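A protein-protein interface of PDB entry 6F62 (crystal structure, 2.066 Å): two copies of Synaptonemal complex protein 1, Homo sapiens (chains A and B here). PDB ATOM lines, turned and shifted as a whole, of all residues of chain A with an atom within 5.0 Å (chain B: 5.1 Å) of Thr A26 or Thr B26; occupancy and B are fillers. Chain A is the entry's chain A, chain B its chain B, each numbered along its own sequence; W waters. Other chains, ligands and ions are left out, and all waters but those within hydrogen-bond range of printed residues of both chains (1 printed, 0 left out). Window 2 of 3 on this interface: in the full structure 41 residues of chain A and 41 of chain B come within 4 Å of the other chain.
Water W1 lies within hydrogen-bond range of NE1 of Trp B22 (3.2 Å) and OE2 of Glu A27 (3.4 Å).
Lys A21 touches none of the printed residues of chain B. Of the printed residues of chain B, Thr A26 touches Thr B26. Of the printed residues of chain A, Trp B22 touches Trp A22 (3.3 Å) and Lys A23 (3.7 Å). Glu B27 touches none of the printed residues of chain A. Of the printed residues of chain A, Glu B29 touches Leu A30 (3.8 Å). Of the printed residues of chain A, Leu B30 touches Glu A29 (3.8 Å) and Leu A30 (3.5 Å). The nearest residue of chain B that does not touch Thr A26 is Leu B30 (4.3 Å). The nearest residue of chain A that does not touch Thr B26 is Leu A30 (4.3 Å).
Trp A22 touches Lys B23, and with the chains exchanged Lys A23 touches Trp B22. Trp A22 touches Thr B26, but with the chains exchanged Thr A26 does not touch Trp B22 (5.0 Å). Thr A26 touches its own counterpart, Thr B26. Glu A29 touches Leu B30, and with the chains exchanged Leu A30 touches Glu B29. 10 positions are printed for both chains. Of the 8 pairs that touch across the chains among the printed residues, 7 have their exchanged pair printed and touching as well.
Trp A22 touches Trp B22. CH2 of Trp A22 touches CA of Lys B23, at 3.6 Å. Trp A22 touches Thr B26. Lys A23 touches Trp B22 (CB to CH2, 3.7 Å). Thr A26 touches Thr B26 (CB to CG2, 3.6 Å). CD2 of Leu B30 touches CG of Glu A29, 3.8 Å away. CG of Glu B29 touches CD2 of Leu A30, at 3.8 Å. CD2 of Leu A30 touches CD2 of Leu B30, at 3.5 Å.
Of the 10 printed residues of chain A, 5 touch a printed residue of chain B. Hydrophobic or aromatic side chains of chain A within 4 Å of the printed part of chain B: Trp A22 and Leu A30. Of the 10 printed residues of chain B, 5 touch a printed residue of chain A. Among the printed residues, no Asp or Glu carboxylate lies within 4 Å of a Lys or Arg side-chain nitrogen of the other chain.
O of Trp A22 sits at hydrogen-bond distance from OG1 of Thr A26 (2.9 Å). The side-chain hydroxyl of Thr A26 lies within hydrogen-bond range of the backbone carbonyl oxygen of Lys A23 (3.1 Å). The side-chain hydroxyl (OG1) of Thr B26 lies within hydrogen-bond range of the backbone carbonyl oxygen (O) of Trp B22 (3.0 Å).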
ATOM      1  N   LYS A  21      15.245 -14.907  -8.454  1.00  0.00           N
ATOM      2  CA  LYS A  21      14.345 -13.852  -8.002  1.00  0.00           C
ATOM      3  C   LYS A  21      12.959 -14.411  -7.703  1.00  0.00           C
ATOM      4  O   LYS A  21      12.365 -14.105  -6.663  1.00  0.00           O
ATOM      5  CB  LYS A  21      14.273 -12.745  -9.054  1.00  0.00           C
ATOM      6  CG  LYS A  21      15.591 -12.008  -9.255  1.00  0.00           C
ATOM      7  CD  LYS A  21      15.441 -10.817 -10.193  1.00  0.00           C
ATOM      8  CE  LYS A  21      16.738 -10.026 -10.294  1.00  0.00           C
ATOM      9  NZ  LYS A  21      16.595  -8.822 -11.157  1.00  0.00           N
ATOM     10  N   TRP A  22      12.430 -15.240  -8.604  1.00  0.00           N
ATOM     11  CA  TRP A  22      11.117 -15.835  -8.375  1.00  0.00           C
ATOM     12  C   TRP A  22      11.118 -16.699  -7.121  1.00  0.00           C
ATOM     13  O   TRP A  22      10.130 -16.728  -6.377  1.00  0.00           O
ATOM     14  CB  TRP A  22      10.698 -16.659  -9.591  1.00  0.00           C
ATOM     15  CG  TRP A  22       9.252 -17.047  -9.580  1.00  0.00           C
ATOM     16  CD1 TRP A  22       8.199 -16.297 -10.019  1.00  0.00           C
ATOM     17  CD2 TRP A  22       8.696 -18.281  -9.110  1.00  0.00           C
ATOM     18  NE1 TRP A  22       7.023 -16.987  -9.850  1.00  0.00           N
ATOM     19  CE2 TRP A  22       7.301 -18.208  -9.294  1.00  0.00           C
ATOM     20  CE3 TRP A  22       9.243 -19.440  -8.551  1.00  0.00           C
ATOM     21  CZ2 TRP A  22       6.446 -19.247  -8.938  1.00  0.00           C
ATOM     22  CZ3 TRP A  22       8.391 -20.471  -8.199  1.00  0.00           C
ATOM     23  CH2 TRP A  22       7.009 -20.367  -8.393  1.00  0.00           C
ATOM     24  N   LYS A  23      12.218 -17.408  -6.866  1.00  0.00           N
ATOM     25  CA  LYS A  23      12.303 -18.232  -5.664  1.00  0.00           C
ATOM     26  C   LYS A  23      12.317 -17.368  -4.409  1.00  0.00           C
ATOM     27  O   LYS A  23      11.587 -17.639  -3.447  1.00  0.00           O
ATOM     28  CB  LYS A  23      13.549 -19.115  -5.721  1.00  0.00           C
ATOM     29  CG  LYS A  23      13.701 -20.043  -4.524  1.00  0.00           C
ATOM     30  CD  LYS A  23      14.972 -20.866  -4.613  1.00  0.00           C
ATOM     31  CE  LYS A  23      15.055 -21.876  -3.484  1.00  0.00           C
ATOM     32  NZ  LYS A  23      16.273 -22.724  -3.591  1.00  0.00           N
ATOM     33  N   VAL A  24      13.145 -16.320  -4.396  1.00  0.00           N
ATOM     34  CA  VAL A  24      13.251 -15.471  -3.212  1.00  0.00           C
ATOM     35  C   VAL A  24      11.923 -14.777  -2.938  1.00  0.00           C
ATOM     36  O   VAL A  24      11.515 -14.620  -1.780  1.00  0.00           O
ATOM     37  CB  VAL A  24      14.397 -14.454  -3.383  1.00  0.00           C
ATOM     38  CG1 VAL A  24      14.438 -13.469  -2.212  1.00  0.00           C
ATOM     39  CG2 VAL A  24      15.730 -15.169  -3.502  1.00  0.00           C
ATOM     40  N   SER A  25      11.226 -14.355  -3.993  1.00  0.00           N
ATOM     41  CA  SER A  25       9.980 -13.621  -3.813  1.00  0.00           C
ATOM     42  C   SER A  25       8.882 -14.526  -3.266  1.00  0.00           C
ATOM     43  O   SER A  25       8.156 -14.146  -2.339  1.00  0.00           O
ATOM     44  CB  SER A  25       9.548 -12.993  -5.139  1.00  0.00           C
ATOM     45  OG  SER A  25       8.319 -12.302  -4.995  1.00  0.00           O
ATOM     46  N   THR A  26       8.743 -15.727  -3.829  1.00  0.00           N
ATOM     47  CA  THR A  26       7.680 -16.628  -3.392  1.00  0.00           C
ATOM     48  C   THR A  26       7.940 -17.150  -1.984  1.00  0.00           C
ATOM     49  O   THR A  26       6.996 -17.351  -1.211  1.00  0.00           O
ATOM     50  CB  THR A  26       7.536 -17.788  -4.376  1.00  0.00           C
ATOM     51  OG1 THR A  26       8.793 -18.461  -4.522  1.00  0.00           O
ATOM     52  CG2 THR A  26       7.066 -17.280  -5.731  1.00  0.00           C
ATOM     53  N   GLU A  27       9.205 -17.383  -1.631  1.00  0.00           N
ATOM     54  CA  GLU A  27       9.521 -17.806  -0.271  1.00  0.00           C
ATOM     55  C   GLU A  27       9.158 -16.719   0.731  1.00  0.00           C
ATOM     56  O   GLU A  27       8.548 -16.991   1.772  1.00  0.00           O
ATOM     57  CB  GLU A  27      11.001 -18.171  -0.161  1.00  0.00           C
ATOM     58  CG  GLU A  27      11.365 -19.470  -0.865  1.00  0.00           C
ATOM     59  CD  GLU A  27      12.834 -19.822  -0.734  1.00  0.00           C
ATOM     60  OE1 GLU A  27      13.624 -18.954  -0.307  1.00  0.00           O
ATOM     61  OE2 GLU A  27      13.199 -20.973  -1.057  1.00  0.00           O
ATOM     62  N   ALA A  28       9.524 -15.472   0.430  1.00  0.00           N
ATOM     63  CA  ALA A  28       9.166 -14.360   1.302  1.00  0.00           C
ATOM     64  C   ALA A  28       7.655 -14.264   1.471  1.00  0.00           C
ATOM     65  O   ALA A  28       7.150 -14.116   2.590  1.00  0.00           O
ATOM     66  CB  ALA A  28       9.728 -13.055   0.739  1.00  0.00           C
ATOM     67  N   GLU A  29       6.914 -14.344   0.365  1.00  0.00           N
ATOM     68  CA  GLU A  29       5.461 -14.243   0.445  1.00  0.00           C
ATOM     69  C   GLU A  29       4.873 -15.369   1.287  1.00  0.00           C
ATOM     70  O   GLU A  29       3.947 -15.144   2.076  1.00  0.00           O
ATOM     71  CB  GLU A  29       4.860 -14.252  -0.961  1.00  0.00           C
ATOM     72  CG  GLU A  29       3.362 -13.993  -0.991  1.00  0.00           C
ATOM     73  CD  GLU A  29       2.814 -13.880  -2.401  1.00  0.00           C
ATOM     74  OE1 GLU A  29       3.611 -13.943  -3.361  1.00  0.00           O
ATOM     75  OE2 GLU A  29       1.583 -13.727  -2.548  1.00  0.00           O
ATOM     76  N   LEU A  30       5.397 -16.588   1.137  1.00  0.00           N
ATOM     77  CA  LEU A  30       4.888 -17.715   1.916  1.00  0.00           C
ATOM     78  C   LEU A  30       5.093 -17.487   3.410  1.00  0.00           C
ATOM     79  O   LEU A  30       4.181 -17.708   4.214  1.00  0.00           O
ATOM     80  CB  LEU A  30       5.571 -19.011   1.472  1.00  0.00           C
ATOM     81  CG  LEU A  30       5.026 -19.678   0.207  1.00  0.00           C
ATOM     82  CD1 LEU A  30       5.977 -20.760  -0.274  1.00  0.00           C
ATOM     83  CD2 LEU A  30       3.642 -20.264   0.458  1.00  0.00           C
ATOM     84  N   LYS B  21       6.988 -28.194 -12.488  1.00  0.00           N
ATOM     85  CA  LYS B  21       6.401 -28.810 -11.303  1.00  0.00           C
ATOM     86  C   LYS B  21       6.620 -27.931 -10.077  1.00  0.00           C
ATOM     87  O   LYS B  21       5.685 -27.651  -9.318  1.00  0.00           O
ATOM     88  CB  LYS B  21       7.000 -30.201 -11.077  1.00  0.00           C
ATOM     89  CG  LYS B  21       6.500 -31.283 -12.029  1.00  0.00           C
ATOM     90  CD  LYS B  21       7.074 -32.649 -11.653  1.00  0.00           C
ATOM     91  CE  LYS B  21       6.571 -33.763 -12.565  1.00  0.00           C
ATOM     92  NZ  LYS B  21       5.152 -34.135 -12.296  1.00  0.00           N
ATOM     93  N   TRP B  22       7.863 -27.490  -9.867  1.00  0.00           N
ATOM     94  CA  TRP B  22       8.187 -26.672  -8.703  1.00  0.00           C
ATOM     95  C   TRP B  22       7.390 -25.374  -8.696  1.00  0.00           C
ATOM     96  O   TRP B  22       6.964 -24.906  -7.634  1.00  0.00           O
ATOM     97  CB  TRP B  22       9.690 -26.396  -8.676  1.00  0.00           C
ATOM     98  CG  TRP B  22      10.108 -25.339  -7.709  1.00  0.00           C
ATOM     99  CD1 TRP B  22      10.053 -25.402  -6.348  1.00  0.00           C
ATOM    100  CD2 TRP B  22      10.666 -24.060  -8.030  1.00  0.00           C
ATOM    101  NE1 TRP B  22      10.534 -24.236  -5.801  1.00  0.00           N
ATOM    102  CE2 TRP B  22      10.918 -23.397  -6.814  1.00  0.00           C
ATOM    103  CE3 TRP B  22      10.972 -23.411  -9.229  1.00  0.00           C
ATOM    104  CZ2 TRP B  22      11.462 -22.115  -6.761  1.00  0.00           C
ATOM    105  CZ3 TRP B  22      11.511 -22.138  -9.176  1.00  0.00           C
ATOM    106  CH2 TRP B  22      11.751 -21.504  -7.951  1.00  0.00           C
ATOM    107  N   LYS B  23       7.172 -24.778  -9.870  1.00  0.00           N
ATOM    108  CA  LYS B  23       6.379 -23.556  -9.929  1.00  0.00           C
ATOM    109  C   LYS B  23       4.931 -23.821  -9.536  1.00  0.00           C
ATOM    110  O   LYS B  23       4.335 -23.048  -8.776  1.00  0.00           O
ATOM    111  CB  LYS B  23       6.444 -22.946 -11.330  1.00  0.00           C
ATOM    112  CG  LYS B  23       7.760 -22.256 -11.666  1.00  0.00           C
ATOM    113  CD  LYS B  23       7.659 -21.520 -12.996  1.00  0.00           C
ATOM    114  CE  LYS B  23       9.014 -21.035 -13.492  1.00  0.00           C
ATOM    115  NZ  LYS B  23       9.526 -19.860 -12.732  1.00  0.00           N
ATOM    116  N   VAL B  24       4.350 -24.911 -10.041  1.00  0.00           N
ATOM    117  CA  VAL B  24       2.952 -25.220  -9.743  1.00  0.00           C
ATOM    118  C   VAL B  24       2.768 -25.457  -8.249  1.00  0.00           C
ATOM    119  O   VAL B  24       1.834 -24.935  -7.629  1.00  0.00           O
ATOM    120  CB  VAL B  24       2.487 -26.430 -10.573  1.00  0.00           C
ATOM    121  CG1 VAL B  24       1.083 -26.878 -10.162  1.00  0.00           C
ATOM    122  CG2 VAL B  24       2.514 -26.091 -12.055  1.00  0.00           C
ATOM    123  N   SER B  25       3.657 -26.254  -7.647  1.00  0.00           N
ATOM    124  CA  SER B  25       3.529 -26.560  -6.226  1.00  0.00           C
ATOM    125  C   SER B  25       3.572 -25.293  -5.379  1.00  0.00           C
ATOM    126  O   SER B  25       2.786 -25.143  -4.436  1.00  0.00           O
ATOM    127  CB  SER B  25       4.633 -27.526  -5.797  1.00  0.00           C
ATOM    128  OG  SER B  25       4.491 -28.780  -6.438  1.00  0.00           O
ATOM    129  N   THR B  26       4.482 -24.372  -5.701  1.00  0.00           N
ATOM    130  CA  THR B  26       4.603 -23.143  -4.922  1.00  0.00           C
ATOM    131  C   THR B  26       3.335 -22.305  -5.024  1.00  0.00           C
ATOM    132  O   THR B  26       2.815 -21.816  -4.013  1.00  0.00           O
ATOM    133  CB  THR B  26       5.818 -22.342  -5.397  1.00  0.00           C
ATOM    134  OG1 THR B  26       7.002 -23.136  -5.250  1.00  0.00           O
ATOM    135  CG2 THR B  26       5.977 -21.054  -4.591  1.00  0.00           C
ATOM    136  N   GLU B  27       2.821 -22.126  -6.242  1.00  0.00           N
ATOM    137  CA  GLU B  27       1.604 -21.345  -6.421  1.00  0.00           C
ATOM    138  C   GLU B  27       0.414 -22.005  -5.738  1.00  0.00           C
ATOM    139  O   GLU B  27      -0.473 -21.312  -5.229  1.00  0.00           O
ATOM    140  CB  GLU B  27       1.329 -21.149  -7.910  1.00  0.00           C
ATOM    141  CG  GLU B  27       2.463 -20.450  -8.649  1.00  0.00           C
ATOM    142  CD  GLU B  27       2.281 -20.460 -10.154  1.00  0.00           C
ATOM    143  OE1 GLU B  27       2.332 -19.374 -10.768  1.00  0.00           O
ATOM    144  OE2 GLU B  27       2.083 -21.555 -10.722  1.00  0.00           O
ATOM    145  N   ALA B  28       0.382 -23.339  -5.708  1.00  0.00           N
ATOM    146  CA  ALA B  28      -0.689 -24.040  -5.009  1.00  0.00           C
ATOM    147  C   ALA B  28      -0.645 -23.751  -3.514  1.00  0.00           C
ATOM    148  O   ALA B  28      -1.673 -23.458  -2.894  1.00  0.00           O
ATOM    149  CB  ALA B  28      -0.586 -25.543  -5.270  1.00  0.00           C
ATOM    150  N   GLU B  29       0.547 -23.831  -2.916  1.00  0.00           N
ATOM    151  CA  GLU B  29       0.676 -23.572  -1.486  1.00  0.00           C
ATOM    152  C   GLU B  29       0.314 -22.129  -1.156  1.00  0.00           C
ATOM    153  O   GLU B  29      -0.259 -21.851  -0.096  1.00  0.00           O
ATOM    154  CB  GLU B  29       2.098 -23.890  -1.025  1.00  0.00           C
ATOM    155  CG  GLU B  29       2.302 -23.776   0.478  1.00  0.00           C
ATOM    156  CD  GLU B  29       3.692 -24.202   0.908  1.00  0.00           C
ATOM    157  OE1 GLU B  29       4.503 -24.572   0.032  1.00  0.00           O
ATOM    158  OE2 GLU B  29       3.974 -24.169   2.125  1.00  0.00           O
ATOM    159  N   LEU B  30       0.643 -21.195  -2.050  1.00  0.00           N
ATOM    160  CA  LEU B  30       0.272 -19.800  -1.835  1.00  0.00           C
ATOM    161  C   LEU B  30      -1.242 -19.638  -1.804  1.00  0.00           C
ATOM    162  O   LEU B  30      -1.793 -18.998  -0.900  1.00  0.00           O
ATOM    163  CB  LEU B  30       0.886 -18.919  -2.924  1.00  0.00           C
ATOM    164  CG  LEU B  30       2.392 -18.663  -2.826  1.00  0.00           C
ATOM    165  CD1 LEU B  30       2.930 -18.106  -4.137  1.00  0.00           C
ATOM    166  CD2 LEU B  30       2.692 -17.709  -1.681  1.00  0.00           C
HETATM  167  O   HOH W   1      11.070 -22.936  -2.932  1.00  0.00           O
